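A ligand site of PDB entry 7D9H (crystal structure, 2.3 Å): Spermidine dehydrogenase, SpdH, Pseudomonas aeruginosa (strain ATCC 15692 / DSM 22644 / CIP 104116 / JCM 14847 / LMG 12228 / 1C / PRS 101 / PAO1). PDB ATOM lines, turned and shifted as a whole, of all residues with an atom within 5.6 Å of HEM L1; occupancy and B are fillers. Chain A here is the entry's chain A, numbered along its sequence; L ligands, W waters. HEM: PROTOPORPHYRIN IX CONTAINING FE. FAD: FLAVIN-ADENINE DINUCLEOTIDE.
NE of Arg 485 lies within salt-bridge range of O2A of HEM L1 (2.9 Å). NE2 of His 21 binds FE of HEM L1, 2.3 Å away. O2B of FAD L2 lies within hydrogen-bond range of OD1 of Asn 73 (2.7 Å). An oxygen (O1D) of HEM L1 lies within hydrogen-bond range of the side-chain hydroxyl (OH) of Tyr 387 (2.6 Å). ND1 of His 74 sits close to O2B of FAD L2 (3.1 Å). NE2 of His 529 is bound to FE of HEM L1, 2.3 Å away. OH of Tyr 381 lies within hydrogen-bond range of O2B of FAD L2, 3.5 Å away. N6A of FAD L2 sits close to SD of Met 384 (3.8 Å).
OG of Ser 12 sits at hydrogen-bond distance from NE2 of His 74, at 3.0 Å. O of Ser 528 lies within hydrogen-bond range of NH1 of Arg 485, 2.6 Å away. The guanidinium group (NH2) of Arg 526 lies within hydrogen-bond range of the backbone carbonyl oxygen (O) of Ser 12. OG of Ser 486 sits at hydrogen-bond distance from O of Arg 482, 3.4 Å away. O of Ala 16 is in hydrogen-bond range of ND2 of Asn 73 (2.5 Å). A ring nitrogen (ND1) of His 529 sits at hydrogen-bond distance from the side-chain sulfur of Met 383 (3.5 Å). The side-chain hydroxyl (OH) of Tyr 387 lies within hydrogen-bond range of the side-chain amino group (NZ) of Lys 27 (3.0 Å).
Residues that only touch HEM L1: Ser 12 (3.1 Å), Phe 17 (3.3 Å), Ala 20 (3.6 Å), Trp 25 (3.3 Å), Asn 73 (3.4 Å), Tyr 381 (3.7 Å), Met 383 (3.5 Å), Met 384 (3.5 Å), Arg 482 (3.9 Å), Ser 486 (3.6 Å), Tyr 489 (3.6 Å), Arg 526 (2.9 Å) and Ser 528 (2.8 Å). Of the 25 residues printed, 17 come within 4 Å of HEM L1. Along chain A the residues within 4 Å of HEM L1 span positions 12 to 529. The nearest printed residue that does not touch HEM L1 is Gly 24 (4.03 Å).
Water W3 lies within hydrogen-bond range of O2D of HEM L1 and O of Met 383. Water W4 bridges O1A of HEM L1 (2.5 Å) and NE of Arg 482 (2.9 Å). Water W1 lies within hydrogen-bond range of an oxygen (O1D) of HEM L1 (2.5 Å), the backbone carbonyl oxygen of Gly 24 (2.7 Å) and the side-chain hydroxyl of Tyr 387 (3.5 Å). Water W2 bridges an oxygen (O2D) of HEM L1 and the backbone carbonyl oxygen (O) of Ser 401.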
ATOM      1  N   SER A  12      14.260  -2.490  13.800  1.00  0.00           N
ATOM      2  CA  SER A  12      14.006  -1.052  13.736  1.00  0.00           C
ATOM      3  C   SER A  12      15.051  -0.358  14.613  1.00  0.00           C
ATOM      4  O   SER A  12      14.824  -0.092  15.796  1.00  0.00           O
ATOM      5  CB  SER A  12      12.577  -0.717  14.163  1.00  0.00           C
ATOM      6  OG  SER A  12      11.667  -1.073  13.128  1.00  0.00           O
ATOM      7  N   HIS A  13      16.203  -0.083  14.018  1.00  0.00           N
ATOM      8  CA  HIS A  13      17.397   0.408  14.698  1.00  0.00           C
ATOM      9  C   HIS A  13      17.309   1.909  14.951  1.00  0.00           C
ATOM     10  O   HIS A  13      16.513   2.601  14.313  1.00  0.00           O
ATOM     11  CB  HIS A  13      18.621   0.106  13.832  1.00  0.00           C
ATOM     12  CG  HIS A  13      18.484   0.639  12.438  1.00  0.00           C
ATOM     13  ND1 HIS A  13      18.559   1.986  12.141  1.00  0.00           N
ATOM     14  CD2 HIS A  13      18.221   0.008  11.272  1.00  0.00           C
ATOM     15  CE1 HIS A  13      18.355   2.153  10.845  1.00  0.00           C
ATOM     16  NE2 HIS A  13      18.153   0.981  10.296  1.00  0.00           N
ATOM     17  N   ALA A  16      16.073   4.868  12.302  1.00  0.00           N
ATOM     18  CA  ALA A  16      15.038   4.477  11.348  1.00  0.00           C
ATOM     19  C   ALA A  16      13.691   5.162  11.620  1.00  0.00           C
ATOM     20  O   ALA A  16      12.927   5.404  10.685  1.00  0.00           O
ATOM     21  CB  ALA A  16      14.836   2.964  11.359  1.00  0.00           C
ATOM     22  N   PHE A  17      13.384   5.471  12.876  1.00  0.00           N
ATOM     23  CA  PHE A  17      12.035   5.800  13.275  1.00  0.00           C
ATOM     24  C   PHE A  17      11.860   7.215  13.810  1.00  0.00           C
ATOM     25  O   PHE A  17      10.717   7.628  14.028  1.00  0.00           O
ATOM     26  CB  PHE A  17      11.584   4.808  14.346  1.00  0.00           C
ATOM     27  CG  PHE A  17      12.501   4.775  15.529  1.00  0.00           C
ATOM     28  CD1 PHE A  17      12.346   5.687  16.581  1.00  0.00           C
ATOM     29  CD2 PHE A  17      13.552   3.871  15.594  1.00  0.00           C
ATOM     30  CE1 PHE A  17      13.191   5.683  17.664  1.00  0.00           C
ATOM     31  CE2 PHE A  17      14.403   3.855  16.673  1.00  0.00           C
ATOM     32  CZ  PHE A  17      14.227   4.775  17.710  1.00  0.00           C
ATOM     33  N   ALA A  20       9.624   9.530  11.826  1.00  0.00           N
ATOM     34  CA  ALA A  20       8.249   9.032  11.877  1.00  0.00           C
ATOM     35  C   ALA A  20       7.605   9.334  13.222  1.00  0.00           C
ATOM     36  O   ALA A  20       6.423   9.680  13.303  1.00  0.00           O
ATOM     37  CB  ALA A  20       8.223   7.537  11.610  1.00  0.00           C
ATOM     38  N   HIS A  21       8.377   9.239  14.305  1.00  0.00           N
ATOM     39  CA  HIS A  21       7.802   9.540  15.615  1.00  0.00           C
ATOM     40  C   HIS A  21       7.538  11.017  15.808  1.00  0.00           C
ATOM     41  O   HIS A  21       6.630  11.388  16.558  1.00  0.00           O
ATOM     42  CB  HIS A  21       8.700   9.016  16.719  1.00  0.00           C
ATOM     43  CG  HIS A  21       8.518   7.575  16.988  1.00  0.00           C
ATOM     44  ND1 HIS A  21       9.328   6.871  17.844  1.00  0.00           N
ATOM     45  CD2 HIS A  21       7.620   6.686  16.504  1.00  0.00           C
ATOM     46  CE1 HIS A  21       8.930   5.606  17.886  1.00  0.00           C
ATOM     47  NE2 HIS A  21       7.893   5.481  17.083  1.00  0.00           N
ATOM     48  N   GLY A  24       4.155  11.068  14.309  1.00  0.00           N
ATOM     49  CA  GLY A  24       3.155  10.306  15.037  1.00  0.00           C
ATOM     50  C   GLY A  24       2.954  10.720  16.485  1.00  0.00           C
ATOM     51  O   GLY A  24       1.833  10.664  16.991  1.00  0.00           O
ATOM     52  N   TRP A  25       4.023  11.107  17.168  1.00  0.00           N
ATOM     53  CA  TRP A  25       3.926  11.423  18.581  1.00  0.00           C
ATOM     54  C   TRP A  25       3.756  12.916  18.817  1.00  0.00           C
ATOM     55  O   TRP A  25       2.891  13.343  19.602  1.00  0.00           O
ATOM     56  CB  TRP A  25       5.183  10.914  19.312  1.00  0.00           C
ATOM     57  CG  TRP A  25       5.326   9.414  19.343  1.00  0.00           C
ATOM     58  CD1 TRP A  25       4.485   8.488  18.808  1.00  0.00           C
ATOM     59  CD2 TRP A  25       6.385   8.667  19.963  1.00  0.00           C
ATOM     60  NE1 TRP A  25       4.948   7.220  19.044  1.00  0.00           N
ATOM     61  CE2 TRP A  25       6.112   7.307  19.760  1.00  0.00           C
ATOM     62  CE3 TRP A  25       7.553   9.030  20.660  1.00  0.00           C
ATOM     63  CZ2 TRP A  25       6.938   6.289  20.251  1.00  0.00           C
ATOM     64  CZ3 TRP A  25       8.374   8.028  21.141  1.00  0.00           C
ATOM     65  CH2 TRP A  25       8.069   6.668  20.933  1.00  0.00           C
ATOM     66  N   LYS A  27       3.180  15.239  16.334  1.00  0.00           N
ATOM     67  CA  LYS A  27       2.345  15.830  15.294  1.00  0.00           C
ATOM     68  C   LYS A  27       3.089  16.894  14.493  1.00  0.00           C
ATOM     69  O   LYS A  27       2.451  17.720  13.846  1.00  0.00           O
ATOM     70  CB  LYS A  27       1.036  16.405  15.852  1.00  0.00           C
ATOM     71  CG  LYS A  27       0.314  15.465  16.793  1.00  0.00           C
ATOM     72  CD  LYS A  27       0.036  14.109  16.149  1.00  0.00           C
ATOM     73  CE  LYS A  27      -0.614  13.177  17.174  1.00  0.00           C
ATOM     74  NZ  LYS A  27      -0.980  11.875  16.581  1.00  0.00           N
ATOM     75  N   ASN A  73      13.077   3.854   5.006  1.00  0.00           N
ATOM     76  CA  ASN A  73      13.622   4.594   6.142  1.00  0.00           C
ATOM     77  C   ASN A  73      14.652   3.815   6.966  1.00  0.00           C
ATOM     78  O   ASN A  73      15.483   4.422   7.633  1.00  0.00           O
ATOM     79  CB  ASN A  73      12.479   5.054   7.056  1.00  0.00           C
ATOM     80  CG  ASN A  73      11.774   3.909   7.719  1.00  0.00           C
ATOM     81  OD1 ASN A  73      11.123   3.107   7.062  1.00  0.00           O
ATOM     82  ND2 ASN A  73      11.931   3.815   9.019  1.00  0.00           N
ATOM     83  N   HIS A  74      14.615   2.486   6.949  1.00  0.00           N
ATOM     84  CA  HIS A  74      15.670   1.704   7.594  1.00  0.00           C
ATOM     85  C   HIS A  74      16.985   1.866   6.807  1.00  0.00           C
ATOM     86  O   HIS A  74      17.014   2.427   5.708  1.00  0.00           O
ATOM     87  CB  HIS A  74      15.270   0.240   7.683  1.00  0.00           C
ATOM     88  CG  HIS A  74      14.280  -0.079   8.759  1.00  0.00           C
ATOM     89  ND1 HIS A  74      12.918  -0.015   8.563  1.00  0.00           N
ATOM     90  CD2 HIS A  74      14.449  -0.478  10.040  1.00  0.00           C
ATOM     91  CE1 HIS A  74      12.296  -0.354   9.674  1.00  0.00           C
ATOM     92  NE2 HIS A  74      13.199  -0.638  10.594  1.00  0.00           N
ATOM     93  N   TYR A 381       3.982   0.926   6.605  1.00  0.00           N
ATOM     94  CA  TYR A 381       2.969   0.591   7.603  1.00  0.00           C
ATOM     95  C   TYR A 381       1.707   1.401   7.333  1.00  0.00           C
ATOM     96  O   TYR A 381       1.777   2.600   7.048  1.00  0.00           O
ATOM     97  CB  TYR A 381       3.490   0.898   9.009  1.00  0.00           C
ATOM     98  CG  TYR A 381       4.831   0.313   9.383  1.00  0.00           C
ATOM     99  CD1 TYR A 381       5.268  -0.906   8.855  1.00  0.00           C
ATOM    100  CD2 TYR A 381       5.669   0.982  10.256  1.00  0.00           C
ATOM    101  CE1 TYR A 381       6.521  -1.434   9.205  1.00  0.00           C
ATOM    102  CE2 TYR A 381       6.907   0.462  10.607  1.00  0.00           C
ATOM    103  CZ  TYR A 381       7.328  -0.737  10.099  1.00  0.00           C
ATOM    104  OH  TYR A 381       8.550  -1.239  10.470  1.00  0.00           O
ATOM    105  N   MET A 383      -0.684   2.314   9.386  1.00  0.00           N
ATOM    106  CA  MET A 383      -0.829   3.333  10.434  1.00  0.00           C
ATOM    107  C   MET A 383       0.000   4.582  10.157  1.00  0.00           C
ATOM    108  O   MET A 383      -0.310   5.642  10.699  1.00  0.00           O
ATOM    109  CB  MET A 383      -0.401   2.739  11.767  1.00  0.00           C
ATOM    110  CG  MET A 383       0.819   1.832  11.499  1.00  0.00           C
ATOM    111  SD  MET A 383       2.200   1.991  12.543  1.00  0.00           S
ATOM    112  CE  MET A 383       3.129   3.322  11.847  1.00  0.00           C
ATOM    113  N   MET A 384       1.084   4.469   9.377  1.00  0.00           N
ATOM    114  CA  MET A 384       1.904   5.618   8.993  1.00  0.00           C
ATOM    115  C   MET A 384       1.258   6.456   7.899  1.00  0.00           C
ATOM    116  O   MET A 384       1.539   7.649   7.790  1.00  0.00           O
ATOM    117  CB  MET A 384       3.282   5.120   8.536  1.00  0.00           C
ATOM    118  CG  MET A 384       4.298   6.197   8.117  1.00  0.00           C
ATOM    119  SD  MET A 384       5.301   6.879   9.486  1.00  0.00           S
ATOM    120  CE  MET A 384       4.326   8.333   9.940  1.00  0.00           C
ATOM    121  N   TYR A 387      -0.300  10.115   8.233  1.00  0.00           N
ATOM    122  CA  TYR A 387       0.610  11.222   8.472  1.00  0.00           C
ATOM    123  C   TYR A 387       1.308  11.706   7.206  1.00  0.00           C
ATOM    124  O   TYR A 387       1.972  12.738   7.249  1.00  0.00           O
ATOM    125  CB  TYR A 387       1.634  10.846   9.544  1.00  0.00           C
ATOM    126  CG  TYR A 387       0.981  10.523  10.862  1.00  0.00           C
ATOM    127  CD1 TYR A 387       0.594  11.539  11.734  1.00  0.00           C
ATOM    128  CD2 TYR A 387       0.707   9.201  11.237  1.00  0.00           C
ATOM    129  CE1 TYR A 387      -0.027  11.272  12.948  1.00  0.00           C
ATOM    130  CE2 TYR A 387       0.087   8.910  12.450  1.00  0.00           C
ATOM    131  CZ  TYR A 387      -0.281   9.952  13.296  1.00  0.00           C
ATOM    132  OH  TYR A 387      -0.911   9.683  14.470  1.00  0.00           O
ATOM    133  N   SER A 401      -5.577   3.909  10.745  1.00  0.00           N
ATOM    134  CA  SER A 401      -4.977   3.956  12.075  1.00  0.00           C
ATOM    135  C   SER A 401      -5.449   2.834  12.974  1.00  0.00           C
ATOM    136  O   SER A 401      -4.838   2.591  14.023  1.00  0.00           O
ATOM    137  CB  SER A 401      -5.292   5.303  12.746  1.00  0.00           C
ATOM    138  OG  SER A 401      -6.642   5.325  13.169  1.00  0.00           O
ATOM    139  N   VAL A 404      -3.261  -1.643  14.104  1.00  0.00           N
ATOM    140  CA  VAL A 404      -2.296  -1.525  15.174  1.00  0.00           C
ATOM    141  C   VAL A 404      -1.371  -2.743  15.088  1.00  0.00           C
ATOM    142  O   VAL A 404      -1.801  -3.867  15.306  1.00  0.00           O
ATOM    143  CB  VAL A 404      -2.996  -1.433  16.531  1.00  0.00           C
ATOM    144  CG1 VAL A 404      -1.986  -1.398  17.685  1.00  0.00           C
ATOM    145  CG2 VAL A 404      -3.969  -0.231  16.573  1.00  0.00           C
ATOM    146  N   ARG A 482       0.124  -1.939  21.783  1.00  0.00           N
ATOM    147  CA  ARG A 482       0.663  -0.607  22.055  1.00  0.00           C
ATOM    148  C   ARG A 482       1.478  -0.606  23.326  1.00  0.00           C
ATOM    149  O   ARG A 482       2.592  -0.065  23.372  1.00  0.00           O
ATOM    150  CB  ARG A 482      -0.462   0.434  22.159  1.00  0.00           C
ATOM    151  CG  ARG A 482      -1.310   0.620  20.899  1.00  0.00           C
ATOM    152  CD  ARG A 482      -2.317   1.736  21.094  1.00  0.00           C
ATOM    153  NE  ARG A 482      -3.264   1.883  19.980  1.00  0.00           N
ATOM    154  CZ  ARG A 482      -4.552   1.528  20.052  1.00  0.00           C
ATOM    155  NH1 ARG A 482      -5.042   1.003  21.168  1.00  0.00           N
ATOM    156  NH2 ARG A 482      -5.338   1.708  18.997  1.00  0.00           N
ATOM    157  N   ARG A 485       4.748  -2.044  22.815  1.00  0.00           N
ATOM    158  CA  ARG A 485       5.682  -1.090  22.224  1.00  0.00           C
ATOM    159  C   ARG A 485       6.224  -0.108  23.267  1.00  0.00           C
ATOM    160  O   ARG A 485       7.398   0.252  23.217  1.00  0.00           O
ATOM    161  CB  ARG A 485       5.030  -0.322  21.073  1.00  0.00           C
ATOM    162  CG  ARG A 485       5.553  -0.762  19.735  1.00  0.00           C
ATOM    163  CD  ARG A 485       4.999   0.056  18.602  1.00  0.00           C
ATOM    164  NE  ARG A 485       3.540   0.008  18.548  1.00  0.00           N
ATOM    165  CZ  ARG A 485       2.853  -0.983  17.990  1.00  0.00           C
ATOM    166  NH1 ARG A 485       3.485  -2.022  17.453  1.00  0.00           N
ATOM    167  NH2 ARG A 485       1.527  -0.938  17.991  1.00  0.00           N
ATOM    168  N   SER A 486       5.386   0.348  24.211  1.00  0.00           N
ATOM    169  CA  SER A 486       5.916   1.176  25.301  1.00  0.00           C
ATOM    170  C   SER A 486       7.028   0.447  26.051  1.00  0.00           C
ATOM    171  O   SER A 486       8.076   1.035  26.333  1.00  0.00           O
ATOM    172  CB  SER A 486       4.806   1.556  26.267  1.00  0.00           C
ATOM    173  OG  SER A 486       3.781   2.199  25.553  1.00  0.00           O
ATOM    174  N   LEU A 488       9.015  -1.969  24.986  1.00  0.00           N
ATOM    175  CA  LEU A 488      10.215  -2.028  24.161  1.00  0.00           C
ATOM    176  C   LEU A 488      10.911  -0.675  24.107  1.00  0.00           C
ATOM    177  O   LEU A 488      12.140  -0.598  24.220  1.00  0.00           O
ATOM    178  CB  LEU A 488       9.867  -2.504  22.749  1.00  0.00           C
ATOM    179  CG  LEU A 488       9.525  -3.976  22.570  1.00  0.00           C
ATOM    180  CD1 LEU A 488       9.350  -4.272  21.077  1.00  0.00           C
ATOM    181  CD2 LEU A 488      10.617  -4.850  23.202  1.00  0.00           C
ATOM    182  N   TYR A 489      10.135   0.395  23.948  1.00  0.00           N
ATOM    183  CA  TYR A 489      10.735   1.728  23.864  1.00  0.00           C
ATOM    184  C   TYR A 489      11.508   2.068  25.124  1.00  0.00           C
ATOM    185  O   TYR A 489      12.525   2.769  25.061  1.00  0.00           O
ATOM    186  CB  TYR A 489       9.647   2.778  23.595  1.00  0.00           C
ATOM    187  CG  TYR A 489      10.162   4.183  23.350  1.00  0.00           C
ATOM    188  CD1 TYR A 489      10.619   4.576  22.103  1.00  0.00           C
ATOM    189  CD2 TYR A 489      10.177   5.125  24.371  1.00  0.00           C
ATOM    190  CE1 TYR A 489      11.097   5.857  21.867  1.00  0.00           C
ATOM    191  CE2 TYR A 489      10.648   6.418  24.138  1.00  0.00           C
ATOM    192  CZ  TYR A 489      11.099   6.773  22.892  1.00  0.00           C
ATOM    193  OH  TYR A 489      11.573   8.047  22.645  1.00  0.00           O
ATOM    194  N   ARG A 526      14.689  -5.692  16.583  1.00  0.00           N
ATOM    195  CA  ARG A 526      13.575  -5.104  17.336  1.00  0.00           C
ATOM    196  C   ARG A 526      12.468  -4.718  16.361  1.00  0.00           C
ATOM    197  O   ARG A 526      12.538  -3.674  15.707  1.00  0.00           O
ATOM    198  CB  ARG A 526      14.055  -3.884  18.121  1.00  0.00           C
ATOM    199  CG  ARG A 526      12.990  -3.218  18.964  1.00  0.00           C
ATOM    200  CD  ARG A 526      13.564  -2.040  19.733  1.00  0.00           C
ATOM    201  NE  ARG A 526      14.291  -1.142  18.837  1.00  0.00           N
ATOM    202  CZ  ARG A 526      14.965  -0.065  19.242  1.00  0.00           C
ATOM    203  NH1 ARG A 526      15.034   0.242  20.517  1.00  0.00           N
ATOM    204  NH2 ARG A 526      15.591   0.699  18.350  1.00  0.00           N
ATOM    205  N   SER A 528       9.379  -3.334  16.506  1.00  0.00           N
ATOM    206  CA  SER A 528       8.382  -2.581  17.262  1.00  0.00           C
ATOM    207  C   SER A 528       7.032  -2.574  16.552  1.00  0.00           C
ATOM    208  O   SER A 528       5.970  -2.613  17.202  1.00  0.00           O
ATOM    209  CB  SER A 528       8.882  -1.157  17.486  1.00  0.00           C
ATOM    210  OG  SER A 528       9.934  -1.166  18.439  1.00  0.00           O
ATOM    211  N   HIS A 529       7.060  -2.472  15.237  1.00  0.00           N
ATOM    212  CA  HIS A 529       5.875  -2.606  14.408  1.00  0.00           C
ATOM    213  C   HIS A 529       6.106  -3.865  13.583  1.00  0.00           C
ATOM    214  O   HIS A 529       6.645  -3.818  12.480  1.00  0.00           O
ATOM    215  CB  HIS A 529       5.683  -1.352  13.548  1.00  0.00           C
ATOM    216  CG  HIS A 529       5.500  -0.125  14.377  1.00  0.00           C
ATOM    217  ND1 HIS A 529       4.263   0.293  14.834  1.00  0.00           N
ATOM    218  CD2 HIS A 529       6.402   0.745  14.908  1.00  0.00           C
ATOM    219  CE1 HIS A 529       4.407   1.379  15.571  1.00  0.00           C
ATOM    220  NE2 HIS A 529       5.692   1.669  15.635  1.00  0.00           N
HETATM  221  CHA HEM L   1       3.570   4.558  17.478  1.00  0.00           C
HETATM  222  CHB HEM L   1       7.455   2.611  19.710  1.00  0.00           C
HETATM  223  CHC HEM L   1       9.611   2.363  15.390  1.00  0.00           C
HETATM  224  CHD HEM L   1       6.102   4.909  13.331  1.00  0.00           C
HETATM  225  C1A HEM L   1       4.423   4.058  18.439  1.00  0.00           C
HETATM  226  C2A HEM L   1       4.129   3.962  19.851  1.00  0.00           C
HETATM  227  C3A HEM L   1       5.197   3.435  20.478  1.00  0.00           C
HETATM  228  C4A HEM L   1       6.211   3.162  19.476  1.00  0.00           C
HETATM  229  CMA HEM L   1       5.368   3.137  21.995  1.00  0.00           C
HETATM  230  CAA HEM L   1       2.794   4.407  20.463  1.00  0.00           C
HETATM  231  CBA HEM L   1       1.862   3.191  20.478  1.00  0.00           C
HETATM  232  CGA HEM L   1       1.153   3.031  19.150  1.00  0.00           C
HETATM  233  O1A HEM L   1       0.343   3.933  18.778  1.00  0.00           O
HETATM  234  O2A HEM L   1       1.377   1.990  18.457  1.00  0.00           O
HETATM  235  C1B HEM L   1       8.410   2.383  18.753  1.00  0.00           C
HETATM  236  C2B HEM L   1       9.760   1.866  18.932  1.00  0.00           C
HETATM  237  C3B HEM L   1      10.323   1.842  17.715  1.00  0.00           C
HETATM  238  C4B HEM L   1       9.358   2.300  16.736  1.00  0.00           C
HETATM  239  CMB HEM L   1      10.434   1.460  20.266  1.00  0.00           C
HETATM  240  CAB HEM L   1      11.711   1.402  17.251  1.00  0.00           C
HETATM  241  CBB HEM L   1      12.132   0.147  17.385  1.00  0.00           C
HETATM  242  C1C HEM L   1       8.850   2.968  14.420  1.00  0.00           C
HETATM  243  C2C HEM L   1       9.094   2.966  12.987  1.00  0.00           C
HETATM  244  C3C HEM L   1       8.088   3.673  12.437  1.00  0.00           C
HETATM  245  C4C HEM L   1       7.219   4.139  13.495  1.00  0.00           C
HETATM  246  CMC HEM L   1      10.285   2.232  12.314  1.00  0.00           C
HETATM  247  CAC HEM L   1       7.783   4.048  10.974  1.00  0.00           C
HETATM  248  CBC HEM L   1       8.720   3.912  10.041  1.00  0.00           C
HETATM  249  C1D HEM L   1       5.116   5.074  14.298  1.00  0.00           C
HETATM  250  C2D HEM L   1       3.933   5.879  14.145  1.00  0.00           C
HETATM  251  C3D HEM L   1       3.229   5.800  15.271  1.00  0.00           C
HETATM  252  C4D HEM L   1       3.936   4.927  16.193  1.00  0.00           C
HETATM  253  CMD HEM L   1       3.564   6.687  12.885  1.00  0.00           C
HETATM  254  CAD HEM L   1       1.879   6.508  15.483  1.00  0.00           C
HETATM  255  CBD HEM L   1       0.801   5.439  15.452  1.00  0.00           C
HETATM  256  CGD HEM L   1      -0.531   6.112  15.204  1.00  0.00           C
HETATM  257  O1D HEM L   1      -0.615   7.337  15.492  1.00  0.00           O
HETATM  258  O2D HEM L   1      -1.470   5.435  14.716  1.00  0.00           O
HETATM  259  NA  HEM L   1       5.700   3.560  18.256  1.00  0.00           N
HETATM  260  NB  HEM L   1       8.208   2.635  17.398  1.00  0.00           N
HETATM  261  NC  HEM L   1       7.714   3.697  14.688  1.00  0.00           N
HETATM  262  ND  HEM L   1       5.085   4.525  15.561  1.00  0.00           N
HETATM  263 FE   HEM L   1       6.675   3.648  16.398  1.00  0.00          FE
HETATM  264  PA  FAD L   2       7.501  -4.344   5.888  1.00  0.00           P
HETATM  265  O1A FAD L   2       8.491  -5.430   5.732  1.00  0.00           O
HETATM  266  O2A FAD L   2       7.172  -3.874   7.329  1.00  0.00           O
HETATM  267  O5B FAD L   2       7.918  -3.136   4.961  1.00  0.00           O
HETATM  268  C5B FAD L   2       7.380  -1.815   5.160  1.00  0.00           C
HETATM  269  C4B FAD L   2       8.543  -0.864   5.274  1.00  0.00           C
HETATM  270  O4B FAD L   2       8.077   0.505   5.151  1.00  0.00           O
HETATM  271  C3B FAD L   2       9.325  -0.943   6.585  1.00  0.00           C
HETATM  272  O3B FAD L   2      10.727  -1.042   6.394  1.00  0.00           O
HETATM  273  C2B FAD L   2       9.014   0.401   7.248  1.00  0.00           C
HETATM  274  O2B FAD L   2      10.033   0.877   8.131  1.00  0.00           O
HETATM  275  C1B FAD L   2       8.889   1.265   6.009  1.00  0.00           C
HETATM  276  N9A FAD L   2       8.301   2.573   6.272  1.00  0.00           N
HETATM  277  C8A FAD L   2       7.436   2.909   7.290  1.00  0.00           C
HETATM  278  N7A FAD L   2       7.130   4.185   7.341  1.00  0.00           N
HETATM  279  C5A FAD L   2       7.862   4.735   6.295  1.00  0.00           C
HETATM  280  C6A FAD L   2       8.000   6.053   5.813  1.00  0.00           C
HETATM  281  N6A FAD L   2       7.363   7.108   6.341  1.00  0.00           N
HETATM  282  N1A FAD L   2       8.832   6.265   4.772  1.00  0.00           N
HETATM  283  C2A FAD L   2       9.476   5.222   4.242  1.00  0.00           C
HETATM  284  N3A FAD L   2       9.429   3.937   4.613  1.00  0.00           N
HETATM  285  C4A FAD L   2       8.606   3.758   5.645  1.00  0.00           C
HETATM  286  N1  FAD L   2       5.643 -13.733   6.963  1.00  0.00           N
HETATM  287  C2  FAD L   2       5.702 -14.976   6.390  1.00  0.00           C
HETATM  288  O2  FAD L   2       5.075 -15.249   5.361  1.00  0.00           O
HETATM  289  N3  FAD L   2       6.434 -15.969   6.990  1.00  0.00           N
HETATM  290  C4  FAD L   2       7.196 -15.848   8.144  1.00  0.00           C
HETATM  291  O4  FAD L   2       7.826 -16.812   8.556  1.00  0.00           O
HETATM  292  C4X FAD L   2       7.143 -14.516   8.743  1.00  0.00           C
HETATM  293  N5  FAD L   2       7.837 -14.296   9.855  1.00  0.00           N
HETATM  294  C5X FAD L   2       7.790 -13.014  10.405  1.00  0.00           C
HETATM  295  C6  FAD L   2       8.512 -12.743  11.571  1.00  0.00           C
HETATM  296  C7  FAD L   2       8.491 -11.476  12.166  1.00  0.00           C
HETATM  297  C7M FAD L   2       9.278 -11.208  13.416  1.00  0.00           C
HETATM  298  C8  FAD L   2       7.734 -10.454  11.565  1.00  0.00           C
HETATM  299  C8M FAD L   2       7.668  -9.074  12.172  1.00  0.00           C
HETATM  300  C9  FAD L   2       7.008 -10.722  10.408  1.00  0.00           C
HETATM  301  C9A FAD L   2       7.038 -11.985   9.816  1.00  0.00           C
HETATM  302  N10 FAD L   2       6.314 -12.272   8.644  1.00  0.00           N
HETATM  303  C10 FAD L   2       6.339 -13.520   8.080  1.00  0.00           C
HETATM  304  C1' FAD L   2       5.455 -11.259   8.017  1.00  0.00           C
HETATM  305  C2' FAD L   2       6.193 -10.113   7.359  1.00  0.00           C
HETATM  306  O2' FAD L   2       5.647  -8.892   7.864  1.00  0.00           O
HETATM  307  C3' FAD L   2       6.020 -10.229   5.850  1.00  0.00           C
HETATM  308  O3' FAD L   2       6.439 -11.528   5.457  1.00  0.00           O
HETATM  309  C4' FAD L   2       6.807  -9.193   5.060  1.00  0.00           C
HETATM  310  O4' FAD L   2       8.169  -9.234   5.501  1.00  0.00           O
HETATM  311  C5' FAD L   2       6.209  -7.825   5.267  1.00  0.00           C
HETATM  312  O5' FAD L   2       6.434  -7.015   4.093  1.00  0.00           O
HETATM  313  P   FAD L   2       5.757  -5.601   3.948  1.00  0.00           P
HETATM  314  O1P FAD L   2       4.254  -5.869   4.026  1.00  0.00           O
HETATM  315  O2P FAD L   2       6.416  -4.982   2.748  1.00  0.00           O
HETATM  316  O3P FAD L   2       6.118  -4.788   5.257  1.00  0.00           O
HETATM  317  O   HOH W   1       0.307   8.493  17.512  1.00  0.00           O
HETATM  318  O   HOH W   2      -2.260   3.056  15.160  1.00  0.00           O
HETATM  319  O   HOH W   3      -2.427   6.152  12.539  1.00  0.00           O
HETATM  320  O   HOH W   4      -2.005   3.524  18.017  1.00  0.00           O
